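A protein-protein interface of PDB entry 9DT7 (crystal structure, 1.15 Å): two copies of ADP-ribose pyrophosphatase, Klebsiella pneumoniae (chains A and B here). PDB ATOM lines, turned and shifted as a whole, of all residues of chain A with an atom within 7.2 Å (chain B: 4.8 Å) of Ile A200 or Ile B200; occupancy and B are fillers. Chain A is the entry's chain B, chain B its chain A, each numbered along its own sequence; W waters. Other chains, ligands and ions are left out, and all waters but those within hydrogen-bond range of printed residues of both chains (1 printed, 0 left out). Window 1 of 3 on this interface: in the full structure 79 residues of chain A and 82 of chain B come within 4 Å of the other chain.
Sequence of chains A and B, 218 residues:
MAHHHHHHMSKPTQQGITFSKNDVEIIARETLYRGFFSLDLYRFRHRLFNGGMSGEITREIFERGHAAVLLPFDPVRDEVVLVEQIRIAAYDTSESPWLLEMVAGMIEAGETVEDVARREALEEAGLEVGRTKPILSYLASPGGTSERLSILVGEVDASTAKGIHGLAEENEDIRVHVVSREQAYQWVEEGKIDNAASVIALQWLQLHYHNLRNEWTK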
ATOM      1  N   LEU A  71       1.679  16.168  10.240  1.00  0.00           N
ATOM      2  CA  LEU A  71       2.208  16.355   8.898  1.00  0.00           C
ATOM      3  C   LEU A  71       1.951  15.071   8.121  1.00  0.00           C
ATOM      4  O   LEU A  71       2.556  14.055   8.447  1.00  0.00           O
ATOM      5  CB  LEU A  71       3.720  16.628   8.972  1.00  0.00           C
ATOM      6  CG  LEU A  71       4.445  16.590   7.626  1.00  0.00           C
ATOM      7  CD1 LEU A  71       3.940  17.625   6.635  1.00  0.00           C
ATOM      8  CD2 LEU A  71       5.954  16.735   7.808  1.00  0.00           C
ATOM      9  N   MET A 102      -1.433  22.092   8.298  1.00  0.00           N
ATOM     10  CA  MET A 102      -1.373  20.714   8.760  1.00  0.00           C
ATOM     11  C   MET A 102      -2.701  20.314   9.378  1.00  0.00           C
ATOM     12  O   MET A 102      -3.399  21.139   9.988  1.00  0.00           O
ATOM     13  CB  MET A 102      -0.331  20.605   9.870  1.00  0.00           C
ATOM     14  CG  MET A 102       1.033  21.113   9.530  1.00  0.00           C
ATOM     15  SD  MET A 102       1.939  20.144   8.294  1.00  0.00           S
ATOM     16  CE  MET A 102       1.434  20.896   6.715  1.00  0.00           C
ATOM     17  N   ILE A 135       7.803  14.897  15.536  1.00  0.00           N
ATOM     18  CA  ILE A 135       8.620  15.979  14.988  1.00  0.00           C
ATOM     19  C   ILE A 135       9.175  16.776  16.171  1.00  0.00           C
ATOM     20  O   ILE A 135      10.288  16.507  16.614  1.00  0.00           O
ATOM     21  CB  ILE A 135       7.808  16.804  13.935  1.00  0.00           C
ATOM     22  CG1 ILE A 135       7.636  15.977  12.654  1.00  0.00           C
ATOM     23  CG2 ILE A 135       8.505  18.125  13.607  1.00  0.00           C
ATOM     24  CD1 ILE A 135       6.861  16.619  11.583  1.00  0.00           C
ATOM     25  N   LEU A 136       8.364  17.640  16.743  1.00  0.00           N
ATOM     26  CA  LEU A 136       8.742  18.607  17.783  1.00  0.00           C
ATOM     27  C   LEU A 136       7.449  18.944  18.530  1.00  0.00           C
ATOM     28  O   LEU A 136       6.382  18.935  17.913  1.00  0.00           O
ATOM     29  CB  LEU A 136       9.356  19.881  17.172  1.00  0.00           C
ATOM     30  CG  LEU A 136      10.700  19.719  16.451  1.00  0.00           C
ATOM     31  CD1 LEU A 136      11.110  21.030  15.794  1.00  0.00           C
ATOM     32  CD2 LEU A 136      11.810  19.270  17.388  1.00  0.00           C
ATOM     33  N   SER A 137       7.568  19.391  19.781  1.00  0.00           N
ATOM     34  CA  SER A 137       6.467  19.992  20.528  1.00  0.00           C
ATOM     35  C   SER A 137       6.886  21.390  20.930  1.00  0.00           C
ATOM     36  O   SER A 137       7.980  21.565  21.448  1.00  0.00           O
ATOM     37  CB  SER A 137       6.144  19.122  21.741  1.00  0.00           C
ATOM     38  OG  SER A 137       5.211  19.737  22.570  1.00  0.00           O
ATOM     39  N   TYR A 138       6.043  22.386  20.634  1.00  0.00           N
ATOM     40  CA  TYR A 138       6.441  23.771  20.806  1.00  0.00           C
ATOM     41  C   TYR A 138       5.348  24.600  21.441  1.00  0.00           C
ATOM     42  O   TYR A 138       4.159  24.290  21.351  1.00  0.00           O
ATOM     43  CB  TYR A 138       6.873  24.419  19.465  1.00  0.00           C
ATOM     44  CG  TYR A 138       5.740  24.620  18.471  1.00  0.00           C
ATOM     45  CD1 TYR A 138       5.286  23.580  17.654  1.00  0.00           C
ATOM     46  CD2 TYR A 138       5.094  25.823  18.362  1.00  0.00           C
ATOM     47  CE1 TYR A 138       4.214  23.755  16.832  1.00  0.00           C
ATOM     48  CE2 TYR A 138       4.037  26.015  17.503  1.00  0.00           C
ATOM     49  CZ  TYR A 138       3.597  24.969  16.746  1.00  0.00           C
ATOM     50  OH  TYR A 138       2.522  25.115  15.890  1.00  0.00           O
ATOM     51  N   LEU A 139       5.782  25.685  22.079  1.00  0.00           N
ATOM     52  CA  LEU A 139       4.893  26.720  22.611  1.00  0.00           C
ATOM     53  C   LEU A 139       4.638  27.747  21.510  1.00  0.00           C
ATOM     54  O   LEU A 139       5.584  28.349  20.963  1.00  0.00           O
ATOM     55  CB  LEU A 139       5.573  27.350  23.820  1.00  0.00           C
ATOM     56  CG  LEU A 139       5.729  26.411  25.013  1.00  0.00           C
ATOM     57  CD1 LEU A 139       6.829  26.931  25.930  1.00  0.00           C
ATOM     58  CD2 LEU A 139       4.402  26.305  25.793  1.00  0.00           C
ATOM     59  N   ALA A 140       3.380  27.946  21.171  1.00  0.00           N
ATOM     60  CA  ALA A 140       3.033  28.838  20.080  1.00  0.00           C
ATOM     61  C   ALA A 140       3.517  30.261  20.272  1.00  0.00           C
ATOM     62  O   ALA A 140       3.974  30.889  19.314  1.00  0.00           O
ATOM     63  CB  ALA A 140       1.514  28.865  19.846  1.00  0.00           C
ATOM     64  N   ILE A 151       3.694  18.040  17.325  1.00  0.00           N
ATOM     65  CA  ILE A 151       3.650  17.662  15.914  1.00  0.00           C
ATOM     66  C   ILE A 151       4.186  16.250  15.749  1.00  0.00           C
ATOM     67  O   ILE A 151       5.281  15.931  16.253  1.00  0.00           O
ATOM     68  CB  ILE A 151       4.473  18.625  15.025  1.00  0.00           C
ATOM     69  CG1 ILE A 151       4.277  20.104  15.339  1.00  0.00           C
ATOM     70  CG2 ILE A 151       4.180  18.328  13.549  1.00  0.00           C
ATOM     71  CD1 ILE A 151       5.258  20.994  14.630  1.00  0.00           C
ATOM     72  N   VAL A 188       6.311  27.555   1.608  1.00  0.00           N
ATOM     73  CA  VAL A 188       6.819  28.184   2.833  1.00  0.00           C
ATOM     74  C   VAL A 188       7.748  29.336   2.501  1.00  0.00           C
ATOM     75  O   VAL A 188       7.607  30.451   3.008  1.00  0.00           O
ATOM     76  CB  VAL A 188       7.507  27.144   3.730  1.00  0.00           C
ATOM     77  CG1 VAL A 188       8.220  27.827   4.858  1.00  0.00           C
ATOM     78  CG2 VAL A 188       6.495  26.175   4.291  1.00  0.00           C
ATOM     79  N   ASN A 195       1.753  29.728   8.657  1.00  0.00           N
ATOM     80  CA  ASN A 195       1.313  29.458  10.022  1.00  0.00           C
ATOM     81  C   ASN A 195       2.367  28.601  10.703  1.00  0.00           C
ATOM     82  O   ASN A 195       3.000  27.751  10.067  1.00  0.00           O
ATOM     83  CB  ASN A 195      -0.067  28.788  10.031  1.00  0.00           C
ATOM     84  CG  ASN A 195      -0.126  27.516   9.216  1.00  0.00           C
ATOM     85  OD1 ASN A 195       0.069  26.427   9.742  1.00  0.00           O
ATOM     86  ND2 ASN A 195      -0.360  27.648   7.903  1.00  0.00           N
ATOM     87  N   ALA A 196       2.584  28.844  11.998  1.00  0.00           N
ATOM     88  CA  ALA A 196       3.695  28.238  12.699  1.00  0.00           C
ATOM     89  C   ALA A 196       3.749  26.721  12.561  1.00  0.00           C
ATOM     90  O   ALA A 196       4.827  26.164  12.307  1.00  0.00           O
ATOM     91  CB  ALA A 196       3.651  28.618  14.166  1.00  0.00           C
ATOM     92  N   ALA A 197       2.638  26.015  12.758  1.00  0.00           N
ATOM     93  CA  ALA A 197       2.720  24.561  12.776  1.00  0.00           C
ATOM     94  C   ALA A 197       3.210  24.025  11.440  1.00  0.00           C
ATOM     95  O   ALA A 197       4.001  23.093  11.389  1.00  0.00           O
ATOM     96  CB  ALA A 197       1.340  23.971  13.063  1.00  0.00           C
ATOM     97  N   SER A 198       2.738  24.611  10.352  1.00  0.00           N
ATOM     98  CA  SER A 198       3.105  24.128   9.022  1.00  0.00           C
ATOM     99  C   SER A 198       4.542  24.510   8.672  1.00  0.00           C
ATOM    100  O   SER A 198       5.269  23.723   8.060  1.00  0.00           O
ATOM    101  CB  SER A 198       2.181  24.732   7.980  1.00  0.00           C
ATOM    102  OG  SER A 198       0.841  24.343   8.165  1.00  0.00           O
ATOM    103  N   VAL A 199       4.968  25.718   9.057  1.00  0.00           N
ATOM    104  CA  VAL A 199       6.343  26.136   8.827  1.00  0.00           C
ATOM    105  C   VAL A 199       7.286  25.210   9.560  1.00  0.00           C
ATOM    106  O   VAL A 199       8.272  24.733   8.986  1.00  0.00           O
ATOM    107  CB  VAL A 199       6.534  27.618   9.210  1.00  0.00           C
ATOM    108  CG1 VAL A 199       7.994  27.993   9.153  1.00  0.00           C
ATOM    109  CG2 VAL A 199       5.709  28.514   8.294  1.00  0.00           C
ATOM    110  N   ILE A 200       7.012  24.957  10.845  1.00  0.00           N
ATOM    111  CA  ILE A 200       7.900  24.108  11.646  1.00  0.00           C
ATOM    112  C   ILE A 200       7.943  22.702  11.062  1.00  0.00           C
ATOM    113  O   ILE A 200       9.010  22.108  10.906  1.00  0.00           O
ATOM    114  CB  ILE A 200       7.451  24.102  13.116  1.00  0.00           C
ATOM    115  CG1 ILE A 200       7.705  25.496  13.715  1.00  0.00           C
ATOM    116  CG2 ILE A 200       8.161  23.031  13.888  1.00  0.00           C
ATOM    117  CD1 ILE A 200       7.087  25.715  15.100  1.00  0.00           C
ATOM    118  N   ALA A 201       6.770  22.149  10.736  1.00  0.00           N
ATOM    119  CA  ALA A 201       6.735  20.798  10.211  1.00  0.00           C
ATOM    120  C   ALA A 201       7.480  20.662   8.887  1.00  0.00           C
ATOM    121  O   ALA A 201       8.186  19.677   8.661  1.00  0.00           O
ATOM    122  CB  ALA A 201       5.302  20.340  10.061  1.00  0.00           C
ATOM    123  N   LEU A 202       7.293  21.617   7.982  1.00  0.00           N
ATOM    124  CA  LEU A 202       7.871  21.530   6.649  1.00  0.00           C
ATOM    125  C   LEU A 202       9.353  21.857   6.651  1.00  0.00           C
ATOM    126  O   LEU A 202      10.105  21.261   5.872  1.00  0.00           O
ATOM    127  CB  LEU A 202       7.074  22.393   5.667  1.00  0.00           C
ATOM    128  CG  LEU A 202       5.682  21.831   5.377  1.00  0.00           C
ATOM    129  CD1 LEU A 202       4.860  22.843   4.601  1.00  0.00           C
ATOM    130  CD2 LEU A 202       5.763  20.498   4.604  1.00  0.00           C
ATOM    131  N   GLN A 203       9.819  22.768   7.518  1.00  0.00           N
ATOM    132  CA  GLN A 203      11.264  22.924   7.652  1.00  0.00           C
ATOM    133  C   GLN A 203      11.892  21.669   8.248  1.00  0.00           C
ATOM    134  O   GLN A 203      12.947  21.218   7.776  1.00  0.00           O
ATOM    135  CB  GLN A 203      11.613  24.180   8.465  1.00  0.00           C
ATOM    136  CG  GLN A 203      11.238  25.501   7.804  1.00  0.00           C
ATOM    137  CD  GLN A 203      11.842  26.721   8.488  1.00  0.00           C
ATOM    138  OE1 GLN A 203      12.441  27.555   7.814  1.00  0.00           O
ATOM    139  NE2 GLN A 203      11.682  26.836   9.809  1.00  0.00           N
ATOM    140  N   TRP A 204      11.238  21.047   9.233  1.00  0.00           N
ATOM    141  CA  TRP A 204      11.713  19.786   9.747  1.00  0.00           C
ATOM    142  C   TRP A 204      11.792  18.746   8.641  1.00  0.00           C
ATOM    143  O   TRP A 204      12.798  18.036   8.498  1.00  0.00           O
ATOM    144  CB  TRP A 204      10.806  19.279  10.883  1.00  0.00           C
ATOM    145  CG  TRP A 204      11.226  17.966  11.451  1.00  0.00           C
ATOM    146  CD1 TRP A 204      12.004  17.769  12.553  1.00  0.00           C
ATOM    147  CD2 TRP A 204      10.885  16.655  10.965  1.00  0.00           C
ATOM    148  NE1 TRP A 204      12.165  16.433  12.784  1.00  0.00           N
ATOM    149  CE2 TRP A 204      11.508  15.728  11.813  1.00  0.00           C
ATOM    150  CE3 TRP A 204      10.097  16.171   9.911  1.00  0.00           C
ATOM    151  CZ2 TRP A 204      11.385  14.356  11.642  1.00  0.00           C
ATOM    152  CZ3 TRP A 204      10.002  14.812   9.719  1.00  0.00           C
ATOM    153  CH2 TRP A 204      10.646  13.912  10.575  1.00  0.00           C
ATOM    154  N   LEU A 205      10.769  18.675   7.797  1.00  0.00           N
ATOM    155  CA  LEU A 205      10.769  17.691   6.722  1.00  0.00           C
ATOM    156  C   LEU A 205      11.917  17.942   5.762  1.00  0.00           C
ATOM    157  O   LEU A 205      12.568  17.008   5.304  1.00  0.00           O
ATOM    158  CB  LEU A 205       9.422  17.700   6.011  1.00  0.00           C
ATOM    159  CG  LEU A 205       9.257  16.625   4.933  1.00  0.00           C
ATOM    160  CD1 LEU A 205       9.395  15.229   5.442  1.00  0.00           C
ATOM    161  CD2 LEU A 205       7.926  16.816   4.243  1.00  0.00           C
ATOM    162  N   GLN A 206      12.220  19.207   5.468  1.00  0.00           N
ATOM    163  CA  GLN A 206      13.373  19.495   4.613  1.00  0.00           C
ATOM    164  C   GLN A 206      14.680  19.047   5.235  1.00  0.00           C
ATOM    165  O   GLN A 206      15.598  18.674   4.514  1.00  0.00           O
ATOM    166  CB  GLN A 206      13.490  20.982   4.290  1.00  0.00           C
ATOM    167  CG  GLN A 206      12.503  21.468   3.303  1.00  0.00           C
ATOM    168  CD  GLN A 206      12.504  20.633   2.027  1.00  0.00           C
ATOM    169  OE1 GLN A 206      11.741  19.667   1.899  1.00  0.00           O
ATOM    170  NE2 GLN A 206      13.375  20.977   1.100  1.00  0.00           N
ATOM    171  N   LEU A 207      14.794  19.074   6.557  1.00  0.00           N
ATOM    172  CA  LEU A 207      15.990  18.635   7.262  1.00  0.00           C
ATOM    173  C   LEU A 207      16.059  17.135   7.469  1.00  0.00           C
ATOM    174  O   LEU A 207      17.138  16.611   7.758  1.00  0.00           O
ATOM    175  CB  LEU A 207      16.070  19.355   8.608  1.00  0.00           C
ATOM    176  CG  LEU A 207      16.401  20.833   8.473  1.00  0.00           C
ATOM    177  CD1 LEU A 207      16.000  21.612   9.721  1.00  0.00           C
ATOM    178  CD2 LEU A 207      17.904  21.033   8.191  1.00  0.00           C
ATOM    179  N   LEU B 136      11.190  34.794   7.747  1.00  0.00           N
ATOM    180  CA  LEU B 136       9.816  34.417   7.445  1.00  0.00           C
ATOM    181  C   LEU B 136       8.940  35.260   8.352  1.00  0.00           C
ATOM    182  O   LEU B 136       9.374  35.676   9.434  1.00  0.00           O
ATOM    183  CB  LEU B 136       9.528  32.904   7.698  1.00  0.00           C
ATOM    184  CG  LEU B 136      10.338  31.891   6.891  1.00  0.00           C
ATOM    185  CD1 LEU B 136      10.059  30.534   7.478  1.00  0.00           C
ATOM    186  CD2 LEU B 136       9.949  31.927   5.438  1.00  0.00           C
ATOM    187  N   TYR B 138       5.116  34.776  10.180  1.00  0.00           N
ATOM    188  CA  TYR B 138       4.194  33.686  10.438  1.00  0.00           C
ATOM    189  C   TYR B 138       3.121  34.085  11.432  1.00  0.00           C
ATOM    190  O   TYR B 138       3.292  34.977  12.279  1.00  0.00           O
ATOM    191  CB  TYR B 138       4.948  32.415  10.917  1.00  0.00           C
ATOM    192  CG  TYR B 138       5.526  32.547  12.324  1.00  0.00           C
ATOM    193  CD1 TYR B 138       6.770  33.153  12.541  1.00  0.00           C
ATOM    194  CD2 TYR B 138       4.838  32.064  13.437  1.00  0.00           C
ATOM    195  CE1 TYR B 138       7.261  33.307  13.805  1.00  0.00           C
ATOM    196  CE2 TYR B 138       5.353  32.197  14.710  1.00  0.00           C
ATOM    197  CZ  TYR B 138       6.576  32.833  14.875  1.00  0.00           C
ATOM    198  OH  TYR B 138       7.107  33.022  16.133  1.00  0.00           O
ATOM    199  N   ILE B 151      10.253  37.589  11.387  1.00  0.00           N
ATOM    200  CA  ILE B 151      11.597  37.253  11.829  1.00  0.00           C
ATOM    201  C   ILE B 151      12.618  37.757  10.830  1.00  0.00           C
ATOM    202  O   ILE B 151      12.474  37.534   9.616  1.00  0.00           O
ATOM    203  CB  ILE B 151      11.790  35.730  12.013  1.00  0.00           C
ATOM    204  CG1 ILE B 151      10.643  35.018  12.723  1.00  0.00           C
ATOM    205  CG2 ILE B 151      13.115  35.461  12.740  1.00  0.00           C
ATOM    206  CD1 ILE B 151      10.781  33.535  12.678  1.00  0.00           C
ATOM    207  N   ALA B 196       7.995  28.728  19.354  1.00  0.00           N
ATOM    208  CA  ALA B 196       7.866  28.777  17.919  1.00  0.00           C
ATOM    209  C   ALA B 196       8.880  29.683  17.234  1.00  0.00           C
ATOM    210  O   ALA B 196       9.468  29.279  16.222  1.00  0.00           O
ATOM    211  CB  ALA B 196       6.475  29.219  17.526  1.00  0.00           C
ATOM    212  N   ALA B 197       9.065  30.904  17.728  1.00  0.00           N
ATOM    213  CA  ALA B 197       9.925  31.840  17.017  1.00  0.00           C
ATOM    214  C   ALA B 197      11.352  31.300  16.920  1.00  0.00           C
ATOM    215  O   ALA B 197      12.003  31.408  15.876  1.00  0.00           O
ATOM    216  CB  ALA B 197       9.924  33.176  17.739  1.00  0.00           C
ATOM    217  N   SER B 198      11.853  30.717  18.015  1.00  0.00           N
ATOM    218  CA  SER B 198      13.208  30.199  18.023  1.00  0.00           C
ATOM    219  C   SER B 198      13.326  28.934  17.200  1.00  0.00           C
ATOM    220  O   SER B 198      14.344  28.732  16.523  1.00  0.00           O
ATOM    221  CB  SER B 198      13.643  29.906  19.444  1.00  0.00           C
ATOM    222  OG  SER B 198      13.636  31.073  20.252  1.00  0.00           O
ATOM    223  N   VAL B 199      12.327  28.052  17.240  1.00  0.00           N
ATOM    224  CA  VAL B 199      12.360  26.845  16.414  1.00  0.00           C
ATOM    225  C   VAL B 199      12.385  27.212  14.945  1.00  0.00           C
ATOM    226  O   VAL B 199      13.206  26.715  14.184  1.00  0.00           O
ATOM    227  CB  VAL B 199      11.182  25.910  16.759  1.00  0.00           C
ATOM    228  CG1 VAL B 199      11.101  24.781  15.798  1.00  0.00           C
ATOM    229  CG2 VAL B 199      11.275  25.404  18.187  1.00  0.00           C
ATOM    230  N   ILE B 200      11.497  28.112  14.523  1.00  0.00           N
ATOM    231  CA  ILE B 200      11.447  28.510  13.114  1.00  0.00           C
ATOM    232  C   ILE B 200      12.762  29.157  12.689  1.00  0.00           C
ATOM    233  O   ILE B 200      13.326  28.852  11.650  1.00  0.00           O
ATOM    234  CB  ILE B 200      10.240  29.433  12.868  1.00  0.00           C
ATOM    235  CG1 ILE B 200       8.938  28.660  13.066  1.00  0.00           C
ATOM    236  CG2 ILE B 200      10.328  30.100  11.519  1.00  0.00           C
ATOM    237  CD1 ILE B 200       7.684  29.529  13.090  1.00  0.00           C
ATOM    238  N   ALA B 201      13.270  30.069  13.509  1.00  0.00           N
ATOM    239  CA  ALA B 201      14.485  30.778  13.154  1.00  0.00           C
ATOM    240  C   ALA B 201      15.681  29.837  13.080  1.00  0.00           C
ATOM    241  O   ALA B 201      16.503  29.943  12.161  1.00  0.00           O
ATOM    242  CB  ALA B 201      14.748  31.886  14.155  1.00  0.00           C
ATOM    243  N   LEU B 202      15.800  28.920  14.031  1.00  0.00           N
ATOM    244  CA  LEU B 202      16.963  28.034  14.065  1.00  0.00           C
ATOM    245  C   LEU B 202      16.878  26.923  13.019  1.00  0.00           C
ATOM    246  O   LEU B 202      17.908  26.500  12.496  1.00  0.00           O
ATOM    247  CB  LEU B 202      17.187  27.472  15.462  1.00  0.00           C
ATOM    248  CG  LEU B 202      17.658  28.531  16.471  1.00  0.00           C
ATOM    249  CD1 LEU B 202      17.558  27.999  17.891  1.00  0.00           C
ATOM    250  CD2 LEU B 202      19.084  29.029  16.151  1.00  0.00           C
ATOM    251  N   GLN B 203      15.676  26.425  12.697  1.00  0.00           N
ATOM    252  CA  GLN B 203      15.521  25.530  11.550  1.00  0.00           C
ATOM    253  C   GLN B 203      15.913  26.225  10.255  1.00  0.00           C
ATOM    254  O   GLN B 203      16.621  25.660   9.423  1.00  0.00           O
ATOM    255  CB  GLN B 203      14.065  25.089  11.414  1.00  0.00           C
ATOM    256  CG  GLN B 203      13.553  24.170  12.445  1.00  0.00           C
ATOM    257  CD  GLN B 203      12.105  23.859  12.230  1.00  0.00           C
ATOM    258  OE1 GLN B 203      11.318  24.727  11.914  1.00  0.00           O
ATOM    259  NE2 GLN B 203      11.749  22.597  12.367  1.00  0.00           N
ATOM    260  N   TRP B 204      15.446  27.459  10.082  1.00  0.00           N
ATOM    261  CA  TRP B 204      15.835  28.254   8.930  1.00  0.00           C
ATOM    262  C   TRP B 204      17.349  28.383   8.881  1.00  0.00           C
ATOM    263  O   TRP B 204      17.979  28.165   7.833  1.00  0.00           O
ATOM    264  CB  TRP B 204      15.168  29.626   8.958  1.00  0.00           C
ATOM    265  CG  TRP B 204      15.553  30.486   7.781  1.00  0.00           C
ATOM    266  CD1 TRP B 204      14.879  30.616   6.621  1.00  0.00           C
ATOM    267  CD2 TRP B 204      16.701  31.342   7.675  1.00  0.00           C
ATOM    268  NE1 TRP B 204      15.542  31.478   5.791  1.00  0.00           N
ATOM    269  CE2 TRP B 204      16.662  31.949   6.419  1.00  0.00           C
ATOM    270  CE3 TRP B 204      17.743  31.667   8.543  1.00  0.00           C
ATOM    271  CZ2 TRP B 204      17.646  32.850   5.993  1.00  0.00           C
ATOM    272  CZ3 TRP B 204      18.714  32.548   8.117  1.00  0.00           C
ATOM    273  CH2 TRP B 204      18.669  33.118   6.853  1.00  0.00           C
HETATM  274  O   HOH W   1       5.850  32.645  18.434  1.00  0.00           O
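The backbone carbonyl oxygen of Leu A139 is in hydrogen-bond range of the backbone NH of Ala B196.
The backbone carbonyl oxygen (O) of Ile B200 sits at hydrogen-bond distance from the side-chain amide nitrogen (NE2) of Gln A203 (3.2 Å).
The side-chain amide nitrogen of Gln B203 is in hydrogen-bond range of the backbone carbonyl oxygen of Ile A200, 3.1 Å away.
The side-chain amide oxygen (OE1) of Gln B203 lies within hydrogen-bond range of the side-chain amide nitrogen (NE2) of Gln A203 (3.0 Å).
The backbone carbonyl oxygen (O) of Leu B136 sits at hydrogen-bond distance from the backbone NH (N) of Ile B151 (2.9 Å).
OH of Tyr B138 lies close to N of Ala B197 (3.3 Å).
N of Ile A151 sits at hydrogen-bond distance from O of Leu A136 (2.9 Å).
The side-chain hydroxyl (OH) of Tyr A138 lies close to the backbone NH (N) of Ala A197.
Among the printed residues, merely in contact across the chains: Ile A200 with Ile B200, Ala A140 with Ala B196, Trp A204 with Gln B203, Gln A203 with Trp B204, Val A199 with Leu B136, Val A188 with Leu B136, Ala A196 with Tyr B138, Leu A136 with Val B199, Tyr A138 with Ala B196, Leu A136 with Gln B203, Gln A203 with Leu B136, Ile A200 with Val B199 and Val A199 with Ile B200.
Printed residues of chain B within 4 Å of Val A188: Leu B136 (3.7 Å).
Printed residues of chain B within 4 Å of Val A199: Leu B136 and Ile B200.
Of the printed residues of chain B, Ile A200 touches Val B199, Ile B200 and Gln B203.
Of the printed residues of chain B, Trp A204 touches Gln B203.
Gln A206 touches none of the printed residues of chain B.
Of the printed residues of chain A, Trp B204 touches Gln A203 (3.6 Å).
The nearest printed residue of chain B that does not touch Ile A200 is Ala B196 (4.2 Å).
Hydrophobic or aromatic side chains of chain B within 4 Å of the printed part of chain A: Leu B136, Tyr B138, Ala B196, Val B199, Ile B200 and Trp B204.
Of the 23 printed residues of chain A, 10 touch a printed residue of chain B.
Hydrophobic or aromatic side chains of chain A that line the printed part of chain B: Leu A136, Tyr A138, Ala A196, Val A199, Ile A200 and Trp A204.
Among the printed residues, 17 pairs touch across the chains.
Among the printed residues, no Asp or Glu carboxylate lies within 4 Å of a Lys or Arg side-chain nitrogen of the other chain.
Leu A136 touches Gln B203, and with the chains exchanged Gln A203 touches Leu B136.
Val A199 touches Ile B200, and with the chains exchanged Ile A200 touches Val B199.
Ile A200 touches Gln B203, and with the chains exchanged Gln A203 touches Ile B200.
Gln A203 touches Trp B204, and with the chains exchanged Trp A204 touches Gln B203.
12 positions are printed for both chains.
Of the 17 pairs that touch across the chains among the printed residues, 14 have their exchanged pair printed and touching as well.
Water W1 bridges the side-chain hydroxyl of Tyr B138 (2.6 Å) and the backbone carbonyl oxygen of Ala A140 (2.7 Å).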
